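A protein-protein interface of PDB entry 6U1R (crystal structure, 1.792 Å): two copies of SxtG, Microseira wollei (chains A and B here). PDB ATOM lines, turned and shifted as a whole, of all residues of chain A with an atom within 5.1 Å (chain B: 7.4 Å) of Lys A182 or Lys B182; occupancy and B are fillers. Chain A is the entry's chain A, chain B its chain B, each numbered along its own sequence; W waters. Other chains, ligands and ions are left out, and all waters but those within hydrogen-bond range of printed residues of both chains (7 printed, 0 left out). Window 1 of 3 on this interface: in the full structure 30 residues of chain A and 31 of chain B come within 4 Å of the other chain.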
ATOM      1  N   GLU A 148      20.843  -9.092 -30.525  1.00  0.00           N
ATOM      2  CA  GLU A 148      20.411  -7.813 -31.079  1.00  0.00           C
ATOM      3  C   GLU A 148      21.432  -6.737 -30.729  1.00  0.00           C
ATOM      4  O   GLU A 148      21.720  -6.490 -29.547  1.00  0.00           O
ATOM      5  CB  GLU A 148      19.017  -7.430 -30.575  1.00  0.00           C
ATOM      6  CG  GLU A 148      17.975  -8.548 -30.805  1.00  0.00           C
ATOM      7  CD  GLU A 148      16.523  -8.094 -30.750  1.00  0.00           C
ATOM      8  OE1 GLU A 148      16.261  -6.895 -30.490  1.00  0.00           O
ATOM      9  OE2 GLU A 148      15.635  -8.957 -30.966  1.00  0.00           O
ATOM     10  N   TYR A 157      16.558   2.420 -34.325  1.00  0.00           N
ATOM     11  CA  TYR A 157      16.281   1.968 -32.960  1.00  0.00           C
ATOM     12  C   TYR A 157      15.314   0.792 -32.913  1.00  0.00           C
ATOM     13  O   TYR A 157      15.382  -0.037 -31.994  1.00  0.00           O
ATOM     14  CB  TYR A 157      15.665   3.122 -32.179  1.00  0.00           C
ATOM     15  CG  TYR A 157      16.024   3.253 -30.708  1.00  0.00           C
ATOM     16  CD1 TYR A 157      17.342   3.349 -30.295  1.00  0.00           C
ATOM     17  CD2 TYR A 157      15.030   3.379 -29.755  1.00  0.00           C
ATOM     18  CE1 TYR A 157      17.652   3.537 -28.960  1.00  0.00           C
ATOM     19  CE2 TYR A 157      15.316   3.567 -28.438  1.00  0.00           C
ATOM     20  CZ  TYR A 157      16.629   3.661 -28.038  1.00  0.00           C
ATOM     21  OH  TYR A 157      16.867   3.853 -26.691  1.00  0.00           O
ATOM     22  N   PHE A 158      14.367   0.737 -33.845  1.00  0.00           N
ATOM     23  CA  PHE A 158      13.330  -0.285 -33.858  1.00  0.00           C
ATOM     24  C   PHE A 158      13.434  -1.181 -35.083  1.00  0.00           C
ATOM     25  O   PHE A 158      12.448  -1.813 -35.488  1.00  0.00           O
ATOM     26  CB  PHE A 158      11.948   0.369 -33.774  1.00  0.00           C
ATOM     27  CG  PHE A 158      11.695   1.037 -32.458  1.00  0.00           C
ATOM     28  CD1 PHE A 158      11.524   0.274 -31.320  1.00  0.00           C
ATOM     29  CD2 PHE A 158      11.672   2.422 -32.343  1.00  0.00           C
ATOM     30  CE1 PHE A 158      11.312   0.855 -30.088  1.00  0.00           C
ATOM     31  CE2 PHE A 158      11.469   3.013 -31.095  1.00  0.00           C
ATOM     32  CZ  PHE A 158      11.290   2.231 -29.976  1.00  0.00           C
ATOM     33  N   TRP A 161      12.117  -4.907 -35.328  1.00  0.00           N
ATOM     34  CA  TRP A 161      10.697  -5.247 -35.237  1.00  0.00           C
ATOM     35  C   TRP A 161      10.234  -6.123 -36.399  1.00  0.00           C
ATOM     36  O   TRP A 161       9.454  -7.065 -36.198  1.00  0.00           O
ATOM     37  CB  TRP A 161       9.876  -3.961 -35.153  1.00  0.00           C
ATOM     38  CG  TRP A 161       9.778  -3.431 -33.739  1.00  0.00           C
ATOM     39  CD1 TRP A 161      10.609  -3.725 -32.672  1.00  0.00           C
ATOM     40  CD2 TRP A 161       8.775  -2.552 -33.230  1.00  0.00           C
ATOM     41  NE1 TRP A 161      10.171  -3.072 -31.544  1.00  0.00           N
ATOM     42  CE2 TRP A 161       9.049  -2.347 -31.858  1.00  0.00           C
ATOM     43  CE3 TRP A 161       7.665  -1.922 -33.800  1.00  0.00           C
ATOM     44  CZ2 TRP A 161       8.253  -1.535 -31.053  1.00  0.00           C
ATOM     45  CZ3 TRP A 161       6.874  -1.115 -33.001  1.00  0.00           C
ATOM     46  CH2 TRP A 161       7.171  -0.930 -31.641  1.00  0.00           C
ATOM     47  N   ARG A 164      10.709  -9.911 -35.591  1.00  0.00           N
ATOM     48  CA  ARG A 164      10.344 -10.533 -34.321  1.00  0.00           C
ATOM     49  C   ARG A 164       9.485 -11.787 -34.505  1.00  0.00           C
ATOM     50  O   ARG A 164       9.555 -12.701 -33.673  1.00  0.00           O
ATOM     51  CB  ARG A 164       9.636  -9.512 -33.426  1.00  0.00           C
ATOM     52  CG  ARG A 164      10.604  -8.549 -32.709  1.00  0.00           C
ATOM     53  CD  ARG A 164      11.646  -9.281 -31.826  1.00  0.00           C
ATOM     54  NE  ARG A 164      12.682  -8.381 -31.276  1.00  0.00           N
ATOM     55  CZ  ARG A 164      12.439  -7.535 -30.288  1.00  0.00           C
ATOM     56  NH1 ARG A 164      11.219  -7.464 -29.784  1.00  0.00           N
ATOM     57  NH2 ARG A 164      13.389  -6.765 -29.805  1.00  0.00           N
ATOM     58  N   ALA A 179      19.909  -9.490 -26.094  1.00  0.00           N
ATOM     59  CA  ALA A 179      20.107  -8.138 -26.593  1.00  0.00           C
ATOM     60  C   ALA A 179      21.209  -7.459 -25.792  1.00  0.00           C
ATOM     61  O   ALA A 179      21.315  -7.650 -24.576  1.00  0.00           O
ATOM     62  CB  ALA A 179      18.825  -7.314 -26.496  1.00  0.00           C
ATOM     63  N   ALA A 180      22.030  -6.679 -26.469  1.00  0.00           N
ATOM     64  CA  ALA A 180      22.859  -5.733 -25.748  1.00  0.00           C
ATOM     65  C   ALA A 180      21.929  -4.678 -25.148  1.00  0.00           C
ATOM     66  O   ALA A 180      20.862  -4.409 -25.707  1.00  0.00           O
ATOM     67  CB  ALA A 180      23.868  -5.067 -26.672  1.00  0.00           C
ATOM     68  N   PRO A 181      22.291  -4.076 -24.018  1.00  0.00           N
ATOM     69  CA  PRO A 181      21.439  -3.010 -23.469  1.00  0.00           C
ATOM     70  C   PRO A 181      21.161  -1.939 -24.519  1.00  0.00           C
ATOM     71  O   PRO A 181      22.053  -1.515 -25.263  1.00  0.00           O
ATOM     72  CB  PRO A 181      22.255  -2.477 -22.281  1.00  0.00           C
ATOM     73  CG  PRO A 181      23.137  -3.684 -21.867  1.00  0.00           C
ATOM     74  CD  PRO A 181      23.478  -4.335 -23.172  1.00  0.00           C
ATOM     75  N   LYS A 182      19.895  -1.530 -24.620  1.00  0.00           N
ATOM     76  CA  LYS A 182      19.507  -0.607 -25.674  1.00  0.00           C
ATOM     77  C   LYS A 182      20.098   0.762 -25.356  1.00  0.00           C
ATOM     78  O   LYS A 182      19.841   1.288 -24.268  1.00  0.00           O
ATOM     79  CB  LYS A 182      17.974  -0.513 -25.801  1.00  0.00           C
ATOM     80  CG  LYS A 182      17.539   0.129 -27.101  1.00  0.00           C
ATOM     81  CD  LYS A 182      16.130  -0.273 -27.477  1.00  0.00           C
ATOM     82  CE  LYS A 182      15.906  -0.114 -28.954  1.00  0.00           C
ATOM     83  NZ  LYS A 182      16.680  -1.108 -29.737  1.00  0.00           N
ATOM     84  N   PRO A 183      20.886   1.365 -26.244  1.00  0.00           N
ATOM     85  CA  PRO A 183      21.579   2.609 -25.879  1.00  0.00           C
ATOM     86  C   PRO A 183      20.616   3.781 -25.785  1.00  0.00           C
ATOM     87  O   PRO A 183      19.547   3.801 -26.395  1.00  0.00           O
ATOM     88  CB  PRO A 183      22.596   2.800 -27.015  1.00  0.00           C
ATOM     89  CG  PRO A 183      21.966   2.106 -28.203  1.00  0.00           C
ATOM     90  CD  PRO A 183      21.282   0.895 -27.588  1.00  0.00           C
ATOM     91  N   GLN A 184      21.036   4.782 -25.005  1.00  0.00           N
ATOM     92  CA  GLN A 184      20.264   6.006 -24.821  1.00  0.00           C
ATOM     93  C   GLN A 184      20.356   6.916 -26.041  1.00  0.00           C
ATOM     94  O   GLN A 184      19.386   7.610 -26.372  1.00  0.00           O
ATOM     95  CB  GLN A 184      20.761   6.760 -23.578  1.00  0.00           C
ATOM     96  CG  GLN A 184      20.594   6.001 -22.271  1.00  0.00           C
ATOM     97  CD  GLN A 184      20.952   6.832 -21.045  1.00  0.00           C
ATOM     98  OE1 GLN A 184      22.126   7.130 -20.786  1.00  0.00           O
ATOM     99  NE2 GLN A 184      19.942   7.231 -20.299  1.00  0.00           N
ATOM    100  N   GLU B 148      18.604  -6.552 -17.715  1.00  0.00           N
ATOM    101  CA  GLU B 148      17.513  -5.594 -17.865  1.00  0.00           C
ATOM    102  C   GLU B 148      16.252  -6.334 -18.311  1.00  0.00           C
ATOM    103  O   GLU B 148      16.238  -6.990 -19.359  1.00  0.00           O
ATOM    104  CB  GLU B 148      17.866  -4.471 -18.848  1.00  0.00           C
ATOM    105  CG  GLU B 148      19.175  -3.738 -18.504  1.00  0.00           C
ATOM    106  CD  GLU B 148      19.342  -2.386 -19.191  1.00  0.00           C
ATOM    107  OE1 GLU B 148      18.478  -1.956 -19.998  1.00  0.00           O
ATOM    108  OE2 GLU B 148      20.369  -1.738 -18.908  1.00  0.00           O
ATOM    109  N   ALA B 149      15.199  -6.204 -17.512  1.00  0.00           N
ATOM    110  CA  ALA B 149      13.957  -6.947 -17.713  1.00  0.00           C
ATOM    111  C   ALA B 149      13.171  -6.428 -18.922  1.00  0.00           C
ATOM    112  O   ALA B 149      13.144  -5.220 -19.195  1.00  0.00           O
ATOM    113  CB  ALA B 149      13.076  -6.849 -16.471  1.00  0.00           C
ATOM    114  N   PRO B 150      12.483  -7.327 -19.638  1.00  0.00           N
ATOM    115  CA  PRO B 150      11.577  -6.909 -20.720  1.00  0.00           C
ATOM    116  C   PRO B 150      10.192  -6.602 -20.177  1.00  0.00           C
ATOM    117  O   PRO B 150       9.330  -7.487 -20.112  1.00  0.00           O
ATOM    118  CB  PRO B 150      11.560  -8.134 -21.639  1.00  0.00           C
ATOM    119  CG  PRO B 150      11.708  -9.305 -20.683  1.00  0.00           C
ATOM    120  CD  PRO B 150      12.520  -8.794 -19.489  1.00  0.00           C
ATOM    121  N   MET B 151       9.973  -5.365 -19.757  1.00  0.00           N
ATOM    122  CA  MET B 151       8.810  -5.051 -18.938  1.00  0.00           C
ATOM    123  C   MET B 151       7.574  -4.822 -19.796  1.00  0.00           C
ATOM    124  O   MET B 151       7.637  -4.190 -20.853  1.00  0.00           O
ATOM    125  CB  MET B 151       9.094  -3.825 -18.070  1.00  0.00           C
ATOM    126  CG  MET B 151      10.290  -4.020 -17.177  1.00  0.00           C
ATOM    127  SD  MET B 151      10.685  -2.577 -16.156  1.00  0.00           S
ATOM    128  CE  MET B 151       9.420  -2.737 -14.895  1.00  0.00           C
ATOM    129  N   ARG B 156       6.938   2.192 -18.582  1.00  0.00           N
ATOM    130  CA  ARG B 156       8.221   1.924 -17.946  1.00  0.00           C
ATOM    131  C   ARG B 156       9.294   1.540 -18.963  1.00  0.00           C
ATOM    132  O   ARG B 156      10.368   1.079 -18.575  1.00  0.00           O
ATOM    133  CB  ARG B 156       8.040   0.835 -16.885  1.00  0.00           C
ATOM    134  CG  ARG B 156       6.873   1.128 -15.933  1.00  0.00           C
ATOM    135  CD  ARG B 156       6.776   0.142 -14.801  1.00  0.00           C
ATOM    136  NE  ARG B 156       7.802   0.356 -13.782  1.00  0.00           N
ATOM    137  CZ  ARG B 156       7.887  -0.342 -12.652  1.00  0.00           C
ATOM    138  NH1 ARG B 156       7.008  -1.296 -12.378  1.00  0.00           N
ATOM    139  NH2 ARG B 156       8.836  -0.065 -11.775  1.00  0.00           N
ATOM    140  N   TYR B 157       9.036   1.801 -20.251  1.00  0.00           N
ATOM    141  CA  TYR B 157       9.924   1.377 -21.340  1.00  0.00           C
ATOM    142  C   TYR B 157      11.342   1.910 -21.171  1.00  0.00           C
ATOM    143  O   TYR B 157      12.308   1.251 -21.572  1.00  0.00           O
ATOM    144  CB  TYR B 157       9.338   1.876 -22.659  1.00  0.00           C
ATOM    145  CG  TYR B 157       9.522   1.013 -23.900  1.00  0.00           C
ATOM    146  CD1 TYR B 157       9.107  -0.318 -23.924  1.00  0.00           C
ATOM    147  CD2 TYR B 157      10.016   1.569 -25.065  1.00  0.00           C
ATOM    148  CE1 TYR B 157       9.218  -1.087 -25.067  1.00  0.00           C
ATOM    149  CE2 TYR B 157      10.146   0.816 -26.227  1.00  0.00           C
ATOM    150  CZ  TYR B 157       9.745  -0.509 -26.232  1.00  0.00           C
ATOM    151  OH  TYR B 157       9.867  -1.228 -27.418  1.00  0.00           O
ATOM    152  N   PHE B 158      11.490   3.122 -20.632  1.00  0.00           N
ATOM    153  CA  PHE B 158      12.796   3.749 -20.502  1.00  0.00           C
ATOM    154  C   PHE B 158      13.224   3.904 -19.046  1.00  0.00           C
ATOM    155  O   PHE B 158      14.106   4.709 -18.733  1.00  0.00           O
ATOM    156  CB  PHE B 158      12.792   5.082 -21.237  1.00  0.00           C
ATOM    157  CG  PHE B 158      12.671   4.930 -22.735  1.00  0.00           C
ATOM    158  CD1 PHE B 158      13.747   4.459 -23.477  1.00  0.00           C
ATOM    159  CD2 PHE B 158      11.484   5.217 -23.399  1.00  0.00           C
ATOM    160  CE1 PHE B 158      13.660   4.305 -24.845  1.00  0.00           C
ATOM    161  CE2 PHE B 158      11.393   5.074 -24.793  1.00  0.00           C
ATOM    162  CZ  PHE B 158      12.474   4.602 -25.503  1.00  0.00           C
ATOM    163  N   GLU B 159      12.678   3.091 -18.164  1.00  0.00           N
ATOM    164  CA  GLU B 159      12.948   3.286 -16.745  1.00  0.00           C
ATOM    165  C   GLU B 159      14.388   2.945 -16.377  1.00  0.00           C
ATOM    166  O   GLU B 159      14.880   3.409 -15.345  1.00  0.00           O
ATOM    167  CB  GLU B 159      11.974   2.468 -15.916  1.00  0.00           C
ATOM    168  CG  GLU B 159      11.927   2.887 -14.428  1.00  0.00           C
ATOM    169  CD  GLU B 159      10.649   2.440 -13.726  1.00  0.00           C
ATOM    170  OE1 GLU B 159       9.547   2.580 -14.319  1.00  0.00           O
ATOM    171  OE2 GLU B 159      10.742   1.944 -12.566  1.00  0.00           O
ATOM    172  N   ALA B 160      15.086   2.153 -17.188  1.00  0.00           N
ATOM    173  CA  ALA B 160      16.496   1.897 -16.885  1.00  0.00           C
ATOM    174  C   ALA B 160      17.371   3.137 -17.039  1.00  0.00           C
ATOM    175  O   ALA B 160      18.518   3.122 -16.573  1.00  0.00           O
ATOM    176  CB  ALA B 160      17.029   0.786 -17.784  1.00  0.00           C
ATOM    177  N   TRP B 161      16.884   4.187 -17.710  1.00  0.00           N
ATOM    178  CA  TRP B 161      17.731   5.338 -18.046  1.00  0.00           C
ATOM    179  C   TRP B 161      18.329   6.000 -16.808  1.00  0.00           C
ATOM    180  O   TRP B 161      19.472   6.485 -16.842  1.00  0.00           O
ATOM    181  CB  TRP B 161      16.932   6.356 -18.873  1.00  0.00           C
ATOM    182  CG  TRP B 161      16.899   6.000 -20.340  1.00  0.00           C
ATOM    183  CD1 TRP B 161      17.132   4.780 -20.879  1.00  0.00           C
ATOM    184  CD2 TRP B 161      16.654   6.888 -21.436  1.00  0.00           C
ATOM    185  NE1 TRP B 161      17.065   4.844 -22.252  1.00  0.00           N
ATOM    186  CE2 TRP B 161      16.768   6.127 -22.620  1.00  0.00           C
ATOM    187  CE3 TRP B 161      16.369   8.259 -21.532  1.00  0.00           C
ATOM    188  CZ2 TRP B 161      16.594   6.681 -23.891  1.00  0.00           C
ATOM    189  CZ3 TRP B 161      16.192   8.814 -22.789  1.00  0.00           C
ATOM    190  CH2 TRP B 161      16.308   8.027 -23.959  1.00  0.00           C
ATOM    191  N   ARG B 164      21.701   4.229 -15.816  1.00  0.00           N
ATOM    192  CA  ARG B 164      22.713   3.866 -16.796  1.00  0.00           C
ATOM    193  C   ARG B 164      24.111   4.333 -16.400  1.00  0.00           C
ATOM    194  O   ARG B 164      25.089   3.677 -16.757  1.00  0.00           O
ATOM    195  CB  ARG B 164      22.315   4.390 -18.175  1.00  0.00           C
ATOM    196  CG  ARG B 164      21.271   3.480 -18.866  1.00  0.00           C
ATOM    197  CD  ARG B 164      21.848   2.087 -19.224  1.00  0.00           C
ATOM    198  NE  ARG B 164      20.840   1.159 -19.778  1.00  0.00           N
ATOM    199  CZ  ARG B 164      20.514   1.135 -21.069  1.00  0.00           C
ATOM    200  NH1 ARG B 164      21.068   2.009 -21.901  1.00  0.00           N
ATOM    201  NH2 ARG B 164      19.610   0.279 -21.531  1.00  0.00           N
ATOM    202  N   TRP B 177      26.506  -7.561 -18.201  1.00  0.00           N
ATOM    203  CA  TRP B 177      25.380  -6.639 -18.334  1.00  0.00           C
ATOM    204  C   TRP B 177      24.615  -7.008 -19.602  1.00  0.00           C
ATOM    205  O   TRP B 177      25.121  -6.821 -20.709  1.00  0.00           O
ATOM    206  CB  TRP B 177      25.910  -5.201 -18.366  1.00  0.00           C
ATOM    207  CG  TRP B 177      24.906  -4.123 -18.581  1.00  0.00           C
ATOM    208  CD1 TRP B 177      23.582  -4.169 -18.329  1.00  0.00           C
ATOM    209  CD2 TRP B 177      25.176  -2.821 -19.115  1.00  0.00           C
ATOM    210  NE1 TRP B 177      22.989  -2.964 -18.655  1.00  0.00           N
ATOM    211  CE2 TRP B 177      23.952  -2.126 -19.159  1.00  0.00           C
ATOM    212  CE3 TRP B 177      26.340  -2.183 -19.568  1.00  0.00           C
ATOM    213  CZ2 TRP B 177      23.852  -0.831 -19.644  1.00  0.00           C
ATOM    214  CZ3 TRP B 177      26.246  -0.899 -20.046  1.00  0.00           C
ATOM    215  CH2 TRP B 177      25.012  -0.226 -20.081  1.00  0.00           C
ATOM    216  N   ALA B 179      20.555  -7.589 -21.664  1.00  0.00           N
ATOM    217  CA  ALA B 179      19.144  -7.221 -21.753  1.00  0.00           C
ATOM    218  C   ALA B 179      18.355  -8.364 -22.378  1.00  0.00           C
ATOM    219  O   ALA B 179      18.798  -8.977 -23.360  1.00  0.00           O
ATOM    220  CB  ALA B 179      18.934  -5.943 -22.571  1.00  0.00           C
ATOM    221  N   ALA B 180      17.190  -8.658 -21.815  1.00  0.00           N
ATOM    222  CA  ALA B 180      16.221  -9.433 -22.577  1.00  0.00           C
ATOM    223  C   ALA B 180      15.793  -8.610 -23.794  1.00  0.00           C
ATOM    224  O   ALA B 180      15.798  -7.378 -23.744  1.00  0.00           O
ATOM    225  CB  ALA B 180      15.000  -9.788 -21.729  1.00  0.00           C
ATOM    226  N   PRO B 181      15.471  -9.252 -24.915  1.00  0.00           N
ATOM    227  CA  PRO B 181      14.984  -8.498 -26.076  1.00  0.00           C
ATOM    228  C   PRO B 181      13.871  -7.540 -25.668  1.00  0.00           C
ATOM    229  O   PRO B 181      12.950  -7.905 -24.927  1.00  0.00           O
ATOM    230  CB  PRO B 181      14.481  -9.589 -27.022  1.00  0.00           C
ATOM    231  CG  PRO B 181      15.301 -10.804 -26.657  1.00  0.00           C
ATOM    232  CD  PRO B 181      15.538 -10.703 -25.182  1.00  0.00           C
ATOM    233  N   LYS B 182      13.963  -6.311 -26.151  1.00  0.00           N
ATOM    234  CA  LYS B 182      13.040  -5.276 -25.721  1.00  0.00           C
ATOM    235  C   LYS B 182      11.696  -5.541 -26.382  1.00  0.00           C
ATOM    236  O   LYS B 182      11.638  -5.649 -27.615  1.00  0.00           O
ATOM    237  CB  LYS B 182      13.541  -3.886 -26.081  1.00  0.00           C
ATOM    238  CG  LYS B 182      12.773  -2.785 -25.352  1.00  0.00           C
ATOM    239  CD  LYS B 182      13.555  -1.488 -25.270  1.00  0.00           C
ATOM    240  CE  LYS B 182      12.995  -0.586 -24.169  1.00  0.00           C
ATOM    241  NZ  LYS B 182      13.241  -1.134 -22.805  1.00  0.00           N
ATOM    242  N   PRO B 183      10.615  -5.667 -25.629  1.00  0.00           N
ATOM    243  CA  PRO B 183       9.358  -6.116 -26.233  1.00  0.00           C
ATOM    244  C   PRO B 183       8.742  -5.027 -27.091  1.00  0.00           C
ATOM    245  O   PRO B 183       8.979  -3.841 -26.883  1.00  0.00           O
ATOM    246  CB  PRO B 183       8.476  -6.451 -25.020  1.00  0.00           C
ATOM    247  CG  PRO B 183       9.035  -5.559 -23.888  1.00  0.00           C
ATOM    248  CD  PRO B 183      10.522  -5.510 -24.164  1.00  0.00           C
ATOM    249  N   GLN B 184       7.930  -5.452 -28.075  1.00  0.00           N
ATOM    250  CA  GLN B 184       7.220  -4.503 -28.929  1.00  0.00           C
ATOM    251  C   GLN B 184       6.031  -3.856 -28.216  1.00  0.00           C
ATOM    252  O   GLN B 184       5.694  -2.701 -28.514  1.00  0.00           O
ATOM    253  CB  GLN B 184       6.720  -5.205 -30.205  1.00  0.00           C
ATOM    254  CG  GLN B 184       7.801  -5.892 -31.027  1.00  0.00           C
ATOM    255  CD  GLN B 184       7.246  -6.492 -32.326  1.00  0.00           C
ATOM    256  OE1 GLN B 184       6.621  -7.558 -32.318  1.00  0.00           O
ATOM    257  NE2 GLN B 184       7.441  -5.788 -33.432  1.00  0.00           N
ATOM    258  N   LEU B 185       5.366  -4.605 -27.328  1.00  0.00           N
ATOM    259  CA  LEU B 185       4.227  -4.125 -26.540  1.00  0.00           C
ATOM    260  C   LEU B 185       3.075  -3.655 -27.431  1.00  0.00           C
ATOM    261  O   LEU B 185       2.406  -2.659 -27.143  1.00  0.00           O
ATOM    262  CB  LEU B 185       4.649  -3.027 -25.559  1.00  0.00           C
ATOM    263  CG  LEU B 185       5.755  -3.483 -24.596  1.00  0.00           C
ATOM    264  CD1 LEU B 185       6.036  -2.414 -23.535  1.00  0.00           C
ATOM    265  CD2 LEU B 185       5.425  -4.800 -23.931  1.00  0.00           C
ATOM    266  N   GLU B 211       4.421 -12.122 -26.587  1.00  0.00           N
ATOM    267  CA  GLU B 211       5.879 -12.043 -26.593  1.00  0.00           C
ATOM    268  C   GLU B 211       6.401 -12.150 -25.164  1.00  0.00           C
ATOM    269  O   GLU B 211       5.643 -11.965 -24.207  1.00  0.00           O
ATOM    270  CB  GLU B 211       6.335 -10.728 -27.235  1.00  0.00           C
ATOM    271  CG  GLU B 211       5.950  -9.487 -26.406  1.00  0.00           C
ATOM    272  CD  GLU B 211       6.202  -8.190 -27.110  1.00  0.00           C
ATOM    273  OE1 GLU B 211       7.116  -8.128 -27.974  1.00  0.00           O
ATOM    274  OE2 GLU B 211       5.481  -7.212 -26.806  1.00  0.00           O
ATOM    275  N   PRO B 212       7.700 -12.395 -24.980  1.00  0.00           N
ATOM    276  CA  PRO B 212       8.228 -12.536 -23.615  1.00  0.00           C
ATOM    277  C   PRO B 212       8.258 -11.204 -22.865  1.00  0.00           C
ATOM    278  O   PRO B 212       8.847 -10.226 -23.335  1.00  0.00           O
ATOM    279  CB  PRO B 212       9.648 -13.090 -23.829  1.00  0.00           C
ATOM    280  CG  PRO B 212       9.803 -13.346 -25.294  1.00  0.00           C
ATOM    281  CD  PRO B 212       8.730 -12.610 -26.013  1.00  0.00           C
ATOM    282  N   THR B 213       7.634 -11.178 -21.675  1.00  0.00           N
ATOM    283  CA  THR B 213       7.751 -10.053 -20.750  1.00  0.00           C
ATOM    284  C   THR B 213       7.878 -10.593 -19.330  1.00  0.00           C
ATOM    285  O   THR B 213       7.306 -11.639 -18.991  1.00  0.00           O
ATOM    286  CB  THR B 213       6.559  -9.052 -20.837  1.00  0.00           C
ATOM    287  OG1 THR B 213       5.318  -9.712 -20.555  1.00  0.00           O
ATOM    288  CG2 THR B 213       6.489  -8.444 -22.207  1.00  0.00           C
HETATM  289  O   HOH W   1       6.507  -5.922 -36.154  1.00  0.00           O
HETATM  290  O   HOH W   2      17.917  -2.239 -22.671  1.00  0.00           O
HETATM  291  O   HOH W   3      11.624  -3.039 -28.988  1.00  0.00           O
HETATM  292  O   HOH W   4      17.281   2.547 -24.012  1.00  0.00           O
HETATM  293  O   HOH W   5      15.981  -5.429 -28.124  1.00  0.00           O
HETATM  294  O   HOH W   6      19.853   9.112 -18.139  1.00  0.00           O
HETATM  295  O   HOH W   7       9.614  -9.561 -27.879  1.00  0.00           O
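O of Lys B182 is in hydrogen-bond range of NH1 of Arg A164 (2.9 Å).
O of Ala B179 sits at hydrogen-bond distance from N of Ala A179 (3.0 Å).
NH1 of Arg B164 lies within hydrogen-bond range of O of Lys A182, 2.8 Å away.
The side-chain carboxylate (OE1) of Glu A148 is in salt-bridge range of the guanidinium group (NH2) of Arg A164 (3.0 Å).
N of Ala A180 is in hydrogen-bond range of O of Glu A148 (3.1 Å).
The backbone carbonyl oxygen (O) of Pro A183 lies within hydrogen-bond range of the side-chain hydroxyl (OH) of Tyr A157 (2.7 Å).
NH2 of Arg B164 lies within salt-bridge range of OE1 of Glu B148, 2.9 Å away.
The backbone carbonyl oxygen of Glu B148 lies within hydrogen-bond range of the backbone NH of Ala B180, at 3.1 Å.
The backbone NH (N) of Gln B184 lies within hydrogen-bond range of the side-chain carboxylate (OE1) of Glu B211 (2.8 Å).
Among the printed residues, merely in contact across the chains: Pro A181 with Trp B177 (3.2 Å), Gln A184 with Trp B161 (3.3 Å), Trp A161 with Gln B184 (3.3 Å), Lys A182 with Lys B182 (3.6 Å), Phe A158 with Tyr B157 (3.7 Å), Tyr A157 with Phe B158 (3.7 Å), Arg A164 with Gln B184 (3.8 Å), Gln A184 with Arg B164 (3.8 Å), Pro A181 with Arg B164 (3.9 Å), Pro A181 with Glu B148 (3.9 Å), Pro A181 with Ala B179 (3.96 Å), Ala A180 with Ala B179 (3.99 Å), Tyr A157 with Trp B161 (3.99 Å) and Trp A161 with Tyr B157 (3.99 Å).
Of the printed residues of chain B, Lys A182 touches Arg B164 (2.8 Å) and Lys B182 (3.6 Å).
Of the printed residues of chain A, Tyr B157 touches Phe A158 and Trp A161.
Ala B160 touches none of the printed residues of chain A.
Lys B182 touches just these residues of chain A: Arg A164 (2.9 Å) and Lys A182 (3.6 Å).
Pro B183 touches none of the printed residues of chain A.
Of the printed residues of chain A, Gln B184 touches Trp A161 and Arg A164.
Printed residues of chain A that touch a printed residue of chain B: Tyr A157, Phe A158, Trp A161, Arg A164, Ala A179, Ala A180, Pro A181, Lys A182 and Gln A184.
Hydrophobic or aromatic side chains of chain A within 4 Å of the printed part of chain B: Tyr A157, Phe A158, Trp A161, Ala A179 and Pro A181.
Of the 22 printed residues of chain B, 9 touch a printed residue of chain A.
Hydrophobic or aromatic side chains of chain B within 4 Å of the printed part of chain A: Tyr B157, Phe B158, Trp B161, Trp B177 and Ala B179.
Among the printed residues, 17 pairs touch across the chains.
Among the printed residues, no Asp or Glu carboxylate lies within 4 Å of a Lys or Arg side-chain nitrogen of the other chain.
Tyr A157 touches Phe B158, and with the chains exchanged Phe A158 touches Tyr B157.
Arg A164 touches Gln B184, and with the chains exchanged Gln A184 touches Arg B164.
Ala B179 touches its own counterpart, Ala A179.
Pro A181 touches Ala B179, but with the chains exchanged Ala A179 does not touch Pro B181 (4.04 Å).
Positions printed for both chains: 148, 157, 158, 161, 164, 179, 180, 181, 182, 183 and 184.
Of the 17 pairs that touch across the chains among the printed residues, 12 have their exchanged pair printed and touching as well.
Water W2 lies within hydrogen-bond range of OE1 of Glu B148 (2.7 Å), N of Lys A182 (2.9 Å) and NH2 of Arg B164 (3.2 Å).
Water W5 lies within hydrogen-bond range of OE1 of Glu A148 (2.8 Å), N of Lys B182 (3.0 Å) and NH2 of Arg A164 (3.4 Å).
Water W4 lies within hydrogen-bond range of the backbone carbonyl oxygen (O) of Lys A182, the indole nitrogen (NE1) of Trp B161 and the side-chain hydroxyl (OH) of Tyr A157.
Water W6 bridges the side-chain amide nitrogen of Gln A184 (2.9 Å) and the backbone carbonyl oxygen of Trp B161 (3.0 Å).
Water W7 lies within hydrogen-bond range of OE1 of Glu B211 and NH1 of Arg A164.
Water W3 lies within hydrogen-bond range of the indole nitrogen (NE1) of Trp A161 (2.9 Å), the backbone carbonyl oxygen (O) of Lys B182 (2.9 Å), the side-chain hydroxyl (OH) of Tyr B157 (3.0 Å) and the backbone carbonyl oxygen (O) of Pro B183 (3.5 Å).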
